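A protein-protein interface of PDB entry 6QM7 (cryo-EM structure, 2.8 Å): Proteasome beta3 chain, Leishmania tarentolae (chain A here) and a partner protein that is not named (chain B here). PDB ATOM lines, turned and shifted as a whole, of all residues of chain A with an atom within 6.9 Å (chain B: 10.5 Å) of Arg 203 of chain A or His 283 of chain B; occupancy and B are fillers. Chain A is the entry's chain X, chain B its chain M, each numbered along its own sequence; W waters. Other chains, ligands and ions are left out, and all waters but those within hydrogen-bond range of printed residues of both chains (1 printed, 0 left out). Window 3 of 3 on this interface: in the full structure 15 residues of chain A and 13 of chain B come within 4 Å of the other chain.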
ATOM      1  N   GLU A 165      23.225  15.640  39.068  1.00  0.00           N
ATOM      2  CA  GLU A 165      23.883  16.297  37.920  1.00  0.00           C
ATOM      3  C   GLU A 165      24.923  15.358  37.329  1.00  0.00           C
ATOM      4  O   GLU A 165      24.927  15.206  36.100  1.00  0.00           O
ATOM      5  CB  GLU A 165      24.507  17.625  38.326  1.00  0.00           C
ATOM      6  CG  GLU A 165      23.456  18.666  38.656  1.00  0.00           C
ATOM      7  CD  GLU A 165      22.448  18.951  37.550  1.00  0.00           C
ATOM      8  OE1 GLU A 165      21.265  19.233  37.871  1.00  0.00           O
ATOM      9  OE2 GLU A 165      22.853  18.897  36.366  1.00  0.00           O
ATOM     10  N   ALA A 168      23.156  12.276  35.726  1.00  0.00           N
ATOM     11  CA  ALA A 168      22.480  12.703  34.485  1.00  0.00           C
ATOM     12  C   ALA A 168      23.529  12.868  33.387  1.00  0.00           C
ATOM     13  O   ALA A 168      23.386  12.201  32.345  1.00  0.00           O
ATOM     14  CB  ALA A 168      21.705  13.969  34.709  1.00  0.00           C
ATOM     15  N   GLN A 169      24.568  13.671  33.627  1.00  0.00           N
ATOM     16  CA  GLN A 169      25.683  13.885  32.660  1.00  0.00           C
ATOM     17  C   GLN A 169      26.359  12.564  32.292  1.00  0.00           C
ATOM     18  O   GLN A 169      26.797  12.438  31.150  1.00  0.00           O
ATOM     19  CB  GLN A 169      26.746  14.831  33.222  1.00  0.00           C
ATOM     20  CG  GLN A 169      26.274  16.273  33.335  1.00  0.00           C
ATOM     21  CD  GLN A 169      25.625  16.743  32.060  1.00  0.00           C
ATOM     22  OE1 GLN A 169      26.200  16.628  30.981  1.00  0.00           O
ATOM     23  NE2 GLN A 169      24.407  17.239  32.174  1.00  0.00           N
ATOM     24  N   LEU A 172      23.527  10.449  30.160  1.00  0.00           N
ATOM     25  CA  LEU A 172      23.354  11.125  28.838  1.00  0.00           C
ATOM     26  C   LEU A 172      24.590  10.945  27.946  1.00  0.00           C
ATOM     27  O   LEU A 172      24.413  10.595  26.782  1.00  0.00           O
ATOM     28  CB  LEU A 172      23.077  12.619  29.037  1.00  0.00           C
ATOM     29  CG  LEU A 172      21.703  12.975  29.597  1.00  0.00           C
ATOM     30  CD1 LEU A 172      21.570  14.483  29.728  1.00  0.00           C
ATOM     31  CD2 LEU A 172      20.579  12.411  28.737  1.00  0.00           C
ATOM     32  N   SER A 173      25.784  11.205  28.464  1.00  0.00           N
ATOM     33  CA  SER A 173      27.046  11.170  27.693  1.00  0.00           C
ATOM     34  C   SER A 173      27.351   9.741  27.250  1.00  0.00           C
ATOM     35  O   SER A 173      27.795   9.565  26.098  1.00  0.00           O
ATOM     36  CB  SER A 173      28.162  11.780  28.479  1.00  0.00           C
ATOM     37  OG  SER A 173      27.823  13.136  28.783  1.00  0.00           O
ATOM     38  N   CYS A 175      25.028   7.265  26.921  1.00  0.00           N
ATOM     39  CA  CYS A 175      23.924   6.918  25.998  1.00  0.00           C
ATOM     40  C   CYS A 175      24.116   7.590  24.637  1.00  0.00           C
ATOM     41  O   CYS A 175      23.524   7.083  23.670  1.00  0.00           O
ATOM     42  CB  CYS A 175      22.572   7.283  26.600  1.00  0.00           C
ATOM     43  SG  CYS A 175      22.011   6.087  27.847  1.00  0.00           S
ATOM     44  N   ASP A 176      24.893   8.673  24.549  1.00  0.00           N
ATOM     45  CA  ASP A 176      25.162   9.375  23.264  1.00  0.00           C
ATOM     46  C   ASP A 176      26.180   8.588  22.443  1.00  0.00           C
ATOM     47  O   ASP A 176      26.293   8.868  21.240  1.00  0.00           O
ATOM     48  CB  ASP A 176      25.660  10.806  23.462  1.00  0.00           C
ATOM     49  CG  ASP A 176      24.586  11.801  23.890  1.00  0.00           C
ATOM     50  OD1 ASP A 176      23.373  11.423  23.918  1.00  0.00           O
ATOM     51  OD2 ASP A 176      24.976  12.956  24.210  1.00  0.00           O
ATOM     52  N   GLY A 182      19.102   5.517  25.115  1.00  0.00           N
ATOM     53  CA  GLY A 182      18.932   6.978  25.091  1.00  0.00           C
ATOM     54  C   GLY A 182      17.476   7.376  25.063  1.00  0.00           C
ATOM     55  O   GLY A 182      16.670   6.694  25.703  1.00  0.00           O
ATOM     56  N   TYR A 183      17.164   8.437  24.324  1.00  0.00           N
ATOM     57  CA  TYR A 183      15.873   9.164  24.379  1.00  0.00           C
ATOM     58  C   TYR A 183      15.706   9.678  25.806  1.00  0.00           C
ATOM     59  O   TYR A 183      14.643   9.524  26.432  1.00  0.00           O
ATOM     60  CB  TYR A 183      14.752   8.299  23.808  1.00  0.00           C
ATOM     61  CG  TYR A 183      15.053   7.847  22.406  1.00  0.00           C
ATOM     62  CD1 TYR A 183      14.706   8.609  21.305  1.00  0.00           C
ATOM     63  CD2 TYR A 183      15.750   6.680  22.192  1.00  0.00           C
ATOM     64  CE1 TYR A 183      15.016   8.193  20.018  1.00  0.00           C
ATOM     65  CE2 TYR A 183      16.077   6.257  20.915  1.00  0.00           C
ATOM     66  CZ  TYR A 183      15.705   7.007  19.816  1.00  0.00           C
ATOM     67  OH  TYR A 183      16.042   6.535  18.573  1.00  0.00           O
ATOM     68  N   GLY A 184      16.771  10.334  26.262  1.00  0.00           N
ATOM     69  CA  GLY A 184      16.822  10.989  27.570  1.00  0.00           C
ATOM     70  C   GLY A 184      16.957   9.953  28.651  1.00  0.00           C
ATOM     71  O   GLY A 184      17.598   8.912  28.402  1.00  0.00           O
ATOM     72  N   ILE A 200      14.704  13.635  32.116  1.00  0.00           N
ATOM     73  CA  ILE A 200      15.895  14.415  31.680  1.00  0.00           C
ATOM     74  C   ILE A 200      15.847  14.495  30.160  1.00  0.00           C
ATOM     75  O   ILE A 200      15.691  13.432  29.522  1.00  0.00           O
ATOM     76  CB  ILE A 200      17.187  13.732  32.160  1.00  0.00           C
ATOM     77  CG1 ILE A 200      17.293  13.725  33.679  1.00  0.00           C
ATOM     78  CG2 ILE A 200      18.432  14.337  31.546  1.00  0.00           C
ATOM     79  CD1 ILE A 200      18.053  12.525  34.176  1.00  0.00           C
ATOM     80  N   LYS A 201      15.960  15.707  29.619  1.00  0.00           N
ATOM     81  CA  LYS A 201      15.963  15.954  28.159  1.00  0.00           C
ATOM     82  C   LYS A 201      17.312  15.451  27.645  1.00  0.00           C
ATOM     83  O   LYS A 201      18.348  15.888  28.182  1.00  0.00           O
ATOM     84  CB  LYS A 201      15.659  17.425  27.842  1.00  0.00           C
ATOM     85  CG  LYS A 201      16.439  18.046  26.689  1.00  0.00           C
ATOM     86  CD  LYS A 201      15.710  19.162  25.944  1.00  0.00           C
ATOM     87  CE  LYS A 201      16.553  19.811  24.857  1.00  0.00           C
ATOM     88  NZ  LYS A 201      17.206  18.819  23.963  1.00  0.00           N
ATOM     89  N   GLY A 202      17.279  14.523  26.690  1.00  0.00           N
ATOM     90  CA  GLY A 202      18.455  14.067  25.930  1.00  0.00           C
ATOM     91  C   GLY A 202      18.157  14.051  24.445  1.00  0.00           C
ATOM     92  O   GLY A 202      17.113  14.601  24.039  1.00  0.00           O
ATOM     93  N   ARG A 203      19.029  13.425  23.660  1.00  0.00           N
ATOM     94  CA  ARG A 203      18.923  13.385  22.177  1.00  0.00           C
ATOM     95  C   ARG A 203      17.730  12.534  21.719  1.00  0.00           C
ATOM     96  O   ARG A 203      17.129  11.862  22.569  1.00  0.00           O
ATOM     97  CB  ARG A 203      20.205  12.813  21.587  1.00  0.00           C
ATOM     98  CG  ARG A 203      21.403  13.724  21.756  1.00  0.00           C
ATOM     99  CD  ARG A 203      22.540  13.229  20.896  1.00  0.00           C
ATOM    100  NE  ARG A 203      23.052  14.343  20.132  1.00  0.00           N
ATOM    101  CZ  ARG A 203      22.584  14.778  18.966  1.00  0.00           C
ATOM    102  NH1 ARG A 203      23.179  15.813  18.406  1.00  0.00           N
ATOM    103  NH2 ARG A 203      21.575  14.197  18.339  1.00  0.00           N
ATOM    104  N   LYS A 204      17.438  12.561  20.414  1.00  0.00           N
ATOM    105  CA  LYS A 204      16.295  11.865  19.767  1.00  0.00           C
ATOM    106  C   LYS A 204      16.807  10.969  18.635  1.00  0.00           C
ATOM    107  O   LYS A 204      16.231  11.017  17.552  1.00  0.00           O
ATOM    108  CB  LYS A 204      15.312  12.929  19.278  1.00  0.00           C
ATOM    109  CG  LYS A 204      14.762  13.834  20.371  1.00  0.00           C
ATOM    110  CD  LYS A 204      13.992  13.064  21.418  1.00  0.00           C
ATOM    111  CE  LYS A 204      13.080  13.918  22.268  1.00  0.00           C
ATOM    112  NZ  LYS A 204      11.906  13.144  22.735  1.00  0.00           N
ATOM    113  N   ASP A 205      17.780  10.104  18.932  1.00  0.00           N
ATOM    114  CA  ASP A 205      18.871   9.677  18.012  1.00  0.00           C
ATOM    115  C   ASP A 205      19.037   8.141  18.033  1.00  0.00           C
ATOM    116  O   ASP A 205      19.241   7.522  19.105  1.00  0.00           O
ATOM    117  CB  ASP A 205      20.151  10.392  18.462  1.00  0.00           C
ATOM    118  CG  ASP A 205      20.985  11.048  17.379  1.00  0.00           C
ATOM    119  OD1 ASP A 205      20.484  11.172  16.257  1.00  0.00           O
ATOM    120  OD2 ASP A 205      22.133  11.451  17.685  1.00  0.00           O
ATOM    121  OXT ASP A 205      18.992   7.440  16.989  1.00  0.00           O
ATOM    122  N   PRO B 273      33.323   9.009  25.771  1.00  0.00           N
ATOM    123  CA  PRO B 273      32.180   9.676  26.391  1.00  0.00           C
ATOM    124  C   PRO B 273      32.546  10.805  27.352  1.00  0.00           C
ATOM    125  O   PRO B 273      31.807  11.752  27.424  1.00  0.00           O
ATOM    126  CB  PRO B 273      31.520   8.605  27.255  1.00  0.00           C
ATOM    127  CG  PRO B 273      31.937   7.323  26.615  1.00  0.00           C
ATOM    128  CD  PRO B 273      33.321   7.573  26.048  1.00  0.00           C
ATOM    129  N   LEU B 275      35.307  12.646  27.204  1.00  0.00           N
ATOM    130  CA  LEU B 275      35.867  13.757  26.396  1.00  0.00           C
ATOM    131  C   LEU B 275      34.703  14.486  25.730  1.00  0.00           C
ATOM    132  O   LEU B 275      34.697  15.716  25.815  1.00  0.00           O
ATOM    133  CB  LEU B 275      36.879  13.221  25.379  1.00  0.00           C
ATOM    134  CG  LEU B 275      38.144  12.576  25.956  1.00  0.00           C
ATOM    135  CD1 LEU B 275      39.127  12.205  24.852  1.00  0.00           C
ATOM    136  CD2 LEU B 275      38.825  13.469  26.981  1.00  0.00           C
ATOM    137  N   ASP B 276      33.743  13.756  25.155  1.00  0.00           N
ATOM    138  CA  ASP B 276      32.460  14.310  24.639  1.00  0.00           C
ATOM    139  C   ASP B 276      31.834  15.222  25.697  1.00  0.00           C
ATOM    140  O   ASP B 276      31.451  16.344  25.334  1.00  0.00           O
ATOM    141  CB  ASP B 276      31.392  13.251  24.332  1.00  0.00           C
ATOM    142  CG  ASP B 276      31.692  12.264  23.216  1.00  0.00           C
ATOM    143  OD1 ASP B 276      32.530  12.569  22.348  1.00  0.00           O
ATOM    144  OD2 ASP B 276      31.062  11.185  23.220  1.00  0.00           O
ATOM    145  N   CYS B 277      31.683  14.726  26.928  1.00  0.00           N
ATOM    146  CA  CYS B 277      31.011  15.437  28.046  1.00  0.00           C
ATOM    147  C   CYS B 277      31.752  16.745  28.338  1.00  0.00           C
ATOM    148  O   CYS B 277      31.095  17.791  28.344  1.00  0.00           O
ATOM    149  CB  CYS B 277      30.952  14.584  29.310  1.00  0.00           C
ATOM    150  SG  CYS B 277      30.010  15.313  30.678  1.00  0.00           S
ATOM    151  N   LEU B 278      33.074  16.686  28.529  1.00  0.00           N
ATOM    152  CA  LEU B 278      33.869  17.791  29.127  1.00  0.00           C
ATOM    153  C   LEU B 278      34.305  18.808  28.065  1.00  0.00           C
ATOM    154  O   LEU B 278      34.701  19.924  28.459  1.00  0.00           O
ATOM    155  CB  LEU B 278      35.083  17.208  29.859  1.00  0.00           C
ATOM    156  CG  LEU B 278      34.766  16.320  31.064  1.00  0.00           C
ATOM    157  CD1 LEU B 278      36.032  15.975  31.847  1.00  0.00           C
ATOM    158  CD2 LEU B 278      33.716  16.957  31.971  1.00  0.00           C
ATOM    159  N   ILE B 279      34.257  18.448  26.784  1.00  0.00           N
ATOM    160  CA  ILE B 279      34.707  19.337  25.678  1.00  0.00           C
ATOM    161  C   ILE B 279      33.470  19.909  24.977  1.00  0.00           C
ATOM    162  O   ILE B 279      33.389  21.155  24.867  1.00  0.00           O
ATOM    163  CB  ILE B 279      35.656  18.581  24.730  1.00  0.00           C
ATOM    164  CG1 ILE B 279      36.915  18.128  25.474  1.00  0.00           C
ATOM    165  CG2 ILE B 279      35.990  19.424  23.509  1.00  0.00           C
ATOM    166  CD1 ILE B 279      37.744  17.098  24.731  1.00  0.00           C
ATOM    167  N   ASN B 280      32.545  19.052  24.536  1.00  0.00           N
ATOM    168  CA  ASN B 280      31.362  19.448  23.721  1.00  0.00           C
ATOM    169  C   ASN B 280      30.231  19.954  24.631  1.00  0.00           C
ATOM    170  O   ASN B 280      29.442  20.793  24.161  1.00  0.00           O
ATOM    171  CB  ASN B 280      30.903  18.318  22.785  1.00  0.00           C
ATOM    172  CG  ASN B 280      31.878  18.039  21.657  1.00  0.00           C
ATOM    173  OD1 ASN B 280      32.681  18.897  21.289  1.00  0.00           O
ATOM    174  ND2 ASN B 280      31.814  16.843  21.092  1.00  0.00           N
ATOM    175  N   ARG B 281      30.130  19.450  25.865  1.00  0.00           N
ATOM    176  CA  ARG B 281      29.216  19.963  26.921  1.00  0.00           C
ATOM    177  C   ARG B 281      27.764  19.974  26.418  1.00  0.00           C
ATOM    178  O   ARG B 281      26.992  20.817  26.900  1.00  0.00           O
ATOM    179  CB  ARG B 281      29.591  21.395  27.340  1.00  0.00           C
ATOM    180  CG  ARG B 281      31.077  21.729  27.431  1.00  0.00           C
ATOM    181  CD  ARG B 281      31.682  21.509  28.799  1.00  0.00           C
ATOM    182  NE  ARG B 281      31.125  22.389  29.814  1.00  0.00           N
ATOM    183  CZ  ARG B 281      31.438  22.343  31.110  1.00  0.00           C
ATOM    184  NH1 ARG B 281      32.310  21.454  31.565  1.00  0.00           N
ATOM    185  NH2 ARG B 281      30.860  23.187  31.952  1.00  0.00           N
ATOM    186  N   GLN B 282      27.373  19.083  25.504  1.00  0.00           N
ATOM    187  CA  GLN B 282      26.118  19.277  24.721  1.00  0.00           C
ATOM    188  C   GLN B 282      24.891  19.148  25.635  1.00  0.00           C
ATOM    189  O   GLN B 282      23.848  19.732  25.279  1.00  0.00           O
ATOM    190  CB  GLN B 282      26.059  18.380  23.478  1.00  0.00           C
ATOM    191  CG  GLN B 282      25.673  16.931  23.742  1.00  0.00           C
ATOM    192  CD  GLN B 282      25.145  16.236  22.509  1.00  0.00           C
ATOM    193  OE1 GLN B 282      24.122  16.622  21.941  1.00  0.00           O
ATOM    194  NE2 GLN B 282      25.830  15.181  22.097  1.00  0.00           N
ATOM    195  N   HIS B 283      25.001  18.464  26.776  1.00  0.00           N
ATOM    196  CA  HIS B 283      23.897  18.309  27.765  1.00  0.00           C
ATOM    197  C   HIS B 283      24.114  19.211  28.980  1.00  0.00           C
ATOM    198  O   HIS B 283      23.771  18.776  30.090  1.00  0.00           O
ATOM    199  CB  HIS B 283      23.772  16.842  28.173  1.00  0.00           C
ATOM    200  CG  HIS B 283      23.368  15.981  27.032  1.00  0.00           C
ATOM    201  ND1 HIS B 283      22.185  16.191  26.352  1.00  0.00           N
ATOM    202  CD2 HIS B 283      23.989  14.947  26.432  1.00  0.00           C
ATOM    203  CE1 HIS B 283      22.090  15.310  25.381  1.00  0.00           C
ATOM    204  NE2 HIS B 283      23.178  14.527  25.418  1.00  0.00           N
ATOM    205  N   MET B 284      24.644  20.420  28.772  1.00  0.00           N
ATOM    206  CA  MET B 284      24.947  21.391  29.856  1.00  0.00           C
ATOM    207  C   MET B 284      24.385  22.764  29.494  1.00  0.00           C
ATOM    208  O   MET B 284      24.671  23.256  28.393  1.00  0.00           O
ATOM    209  CB  MET B 284      26.449  21.474  30.125  1.00  0.00           C
ATOM    210  CG  MET B 284      26.982  20.184  30.713  1.00  0.00           C
ATOM    211  SD  MET B 284      28.656  20.335  31.353  1.00  0.00           S
ATOM    212  CE  MET B 284      29.148  18.609  31.401  1.00  0.00           C
ATOM    213  N   THR B 285      23.587  23.322  30.408  1.00  0.00           N
ATOM    214  CA  THR B 285      22.905  24.635  30.300  1.00  0.00           C
ATOM    215  C   THR B 285      23.905  25.749  30.638  1.00  0.00           C
ATOM    216  O   THR B 285      23.734  26.862  30.102  1.00  0.00           O
ATOM    217  CB  THR B 285      21.663  24.669  31.203  1.00  0.00           C
ATOM    218  OG1 THR B 285      20.994  23.408  31.130  1.00  0.00           O
ATOM    219  CG2 THR B 285      20.695  25.771  30.824  1.00  0.00           C
ATOM    220  N   SER B 286      24.907  25.453  31.477  1.00  0.00           N
ATOM    221  CA  SER B 286      26.041  26.348  31.847  1.00  0.00           C
ATOM    222  C   SER B 286      26.714  26.916  30.590  1.00  0.00           C
ATOM    223  O   SER B 286      26.711  26.224  29.553  1.00  0.00           O
ATOM    224  CB  SER B 286      27.050  25.622  32.706  1.00  0.00           C
ATOM    225  OG  SER B 286      26.407  24.835  33.699  1.00  0.00           O
ATOM    226  N   GLN B 287      27.271  28.132  30.687  1.00  0.00           N
ATOM    227  CA  GLN B 287      28.061  28.790  29.606  1.00  0.00           C
ATOM    228  C   GLN B 287      29.394  28.046  29.455  1.00  0.00           C
ATOM    229  O   GLN B 287      30.047  27.805  30.496  1.00  0.00           O
ATOM    230  CB  GLN B 287      28.297  30.276  29.910  1.00  0.00           C
ATOM    231  CG  GLN B 287      27.039  31.139  29.836  1.00  0.00           C
ATOM    232  CD  GLN B 287      26.709  31.627  28.444  1.00  0.00           C
ATOM    233  OE1 GLN B 287      26.984  30.967  27.444  1.00  0.00           O
ATOM    234  NE2 GLN B 287      26.098  32.798  28.367  1.00  0.00           N
ATOM    235  N   ALA B 288      29.771  27.696  28.216  1.00  0.00           N
ATOM    236  CA  ALA B 288      30.994  26.930  27.860  1.00  0.00           C
ATOM    237  C   ALA B 288      32.228  27.615  28.455  1.00  0.00           C
ATOM    238  O   ALA B 288      32.406  28.813  28.240  1.00  0.00           O
ATOM    239  CB  ALA B 288      31.105  26.803  26.356  1.00  0.00           C
HETATM  240  O   HOH W   1      27.389  16.742  28.714  1.00  0.00           O
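NE2 of Gln 169 of chain A is in hydrogen-bond range of O of His 283 of chain B (2.7 Å).
SG of Cys 277 of chain B sits close to OG of Ser 173 of chain A (3.6 Å).
OD2 of Asp 176 of chain A lies within hydrogen-bond range of NE2 of Gln 282 of chain B.
NE2 of His 283 of chain B is in hydrogen-bond range of OD2 of Asp 176 of chain A.
NE of Arg 203 of chain A lies within hydrogen-bond range of OE1 of Gln 282 of chain B, at 3.1 Å.
The backbone carbonyl oxygen (O) of Gln 169 of chain A lies within hydrogen-bond range of the side-chain hydroxyl (OG) of Ser 173 of chain A (2.7 Å).
The side-chain carboxylate (OD2) of Asp 205 of chain A is in salt-bridge range of the guanidinium group (NH2) of Arg 203 of chain A, 2.9 Å away.
NE of Arg 281 of chain B sits close to SD of Met 284 of chain B (3.6 Å).
Among the printed residues, pairs that only touch across the chains: Gln 169 of chain A with Met 284 of chain B (3.6 Å), Leu 172 of chain A with His 283 of chain B (3.6 Å), Ser 173 of chain A with Pro 273 of chain B (3.8 Å), Gly 202 of chain A with His 283 of chain B (3.9 Å) and Arg 203 of chain A with His 283 of chain B (3.99 Å).
Of the printed residues of chain B, Arg 203 of chain A touches Gln 282 and His 283.
Printed residues of chain A within 4 Å of His 283 of chain B: Gln 169, Leu 172, Asp 176, Gly 202 and Arg 203.
Of chain B, only His 283 comes within 4 Å of Leu 172 of chain A.
Asp 176 of chain A touches two residues of chain B.
Of chain B, only His 283 comes within 4 Å of Gly 202 of chain A.
No residue of chain B comes within 4 Å of Lys 204 of chain A.
Of the printed residues of chain A, Pro 273 of chain B touches Ser 173.
Of the printed residues of chain B, Gln 169 of chain A touches His 283 and Met 284.
The nearest printed residue of chain B that does not touch Arg 203 of chain A is Asp 276 of chain B (9.1 Å).
The nearest printed residue of chain A that does not touch His 283 of chain B is Lys 201 of chain A (4.3 Å).
Of the 15 printed residues of chain B, 5 touch a printed residue of chain A.
Printed residues of chain B that touch a printed residue of chain A: Pro 273, Cys 277, Gln 282, His 283 and Met 284.
Of the 16 printed residues of chain A, 6 touch a printed residue of chain B.
Among the printed residues, 10 pairs touch across the chains.
Water W1 lies within hydrogen-bond range of OE1 of Gln 169 of chain A (2.6 Å) and SG of Cys 277 of chain B (3.6 Å).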
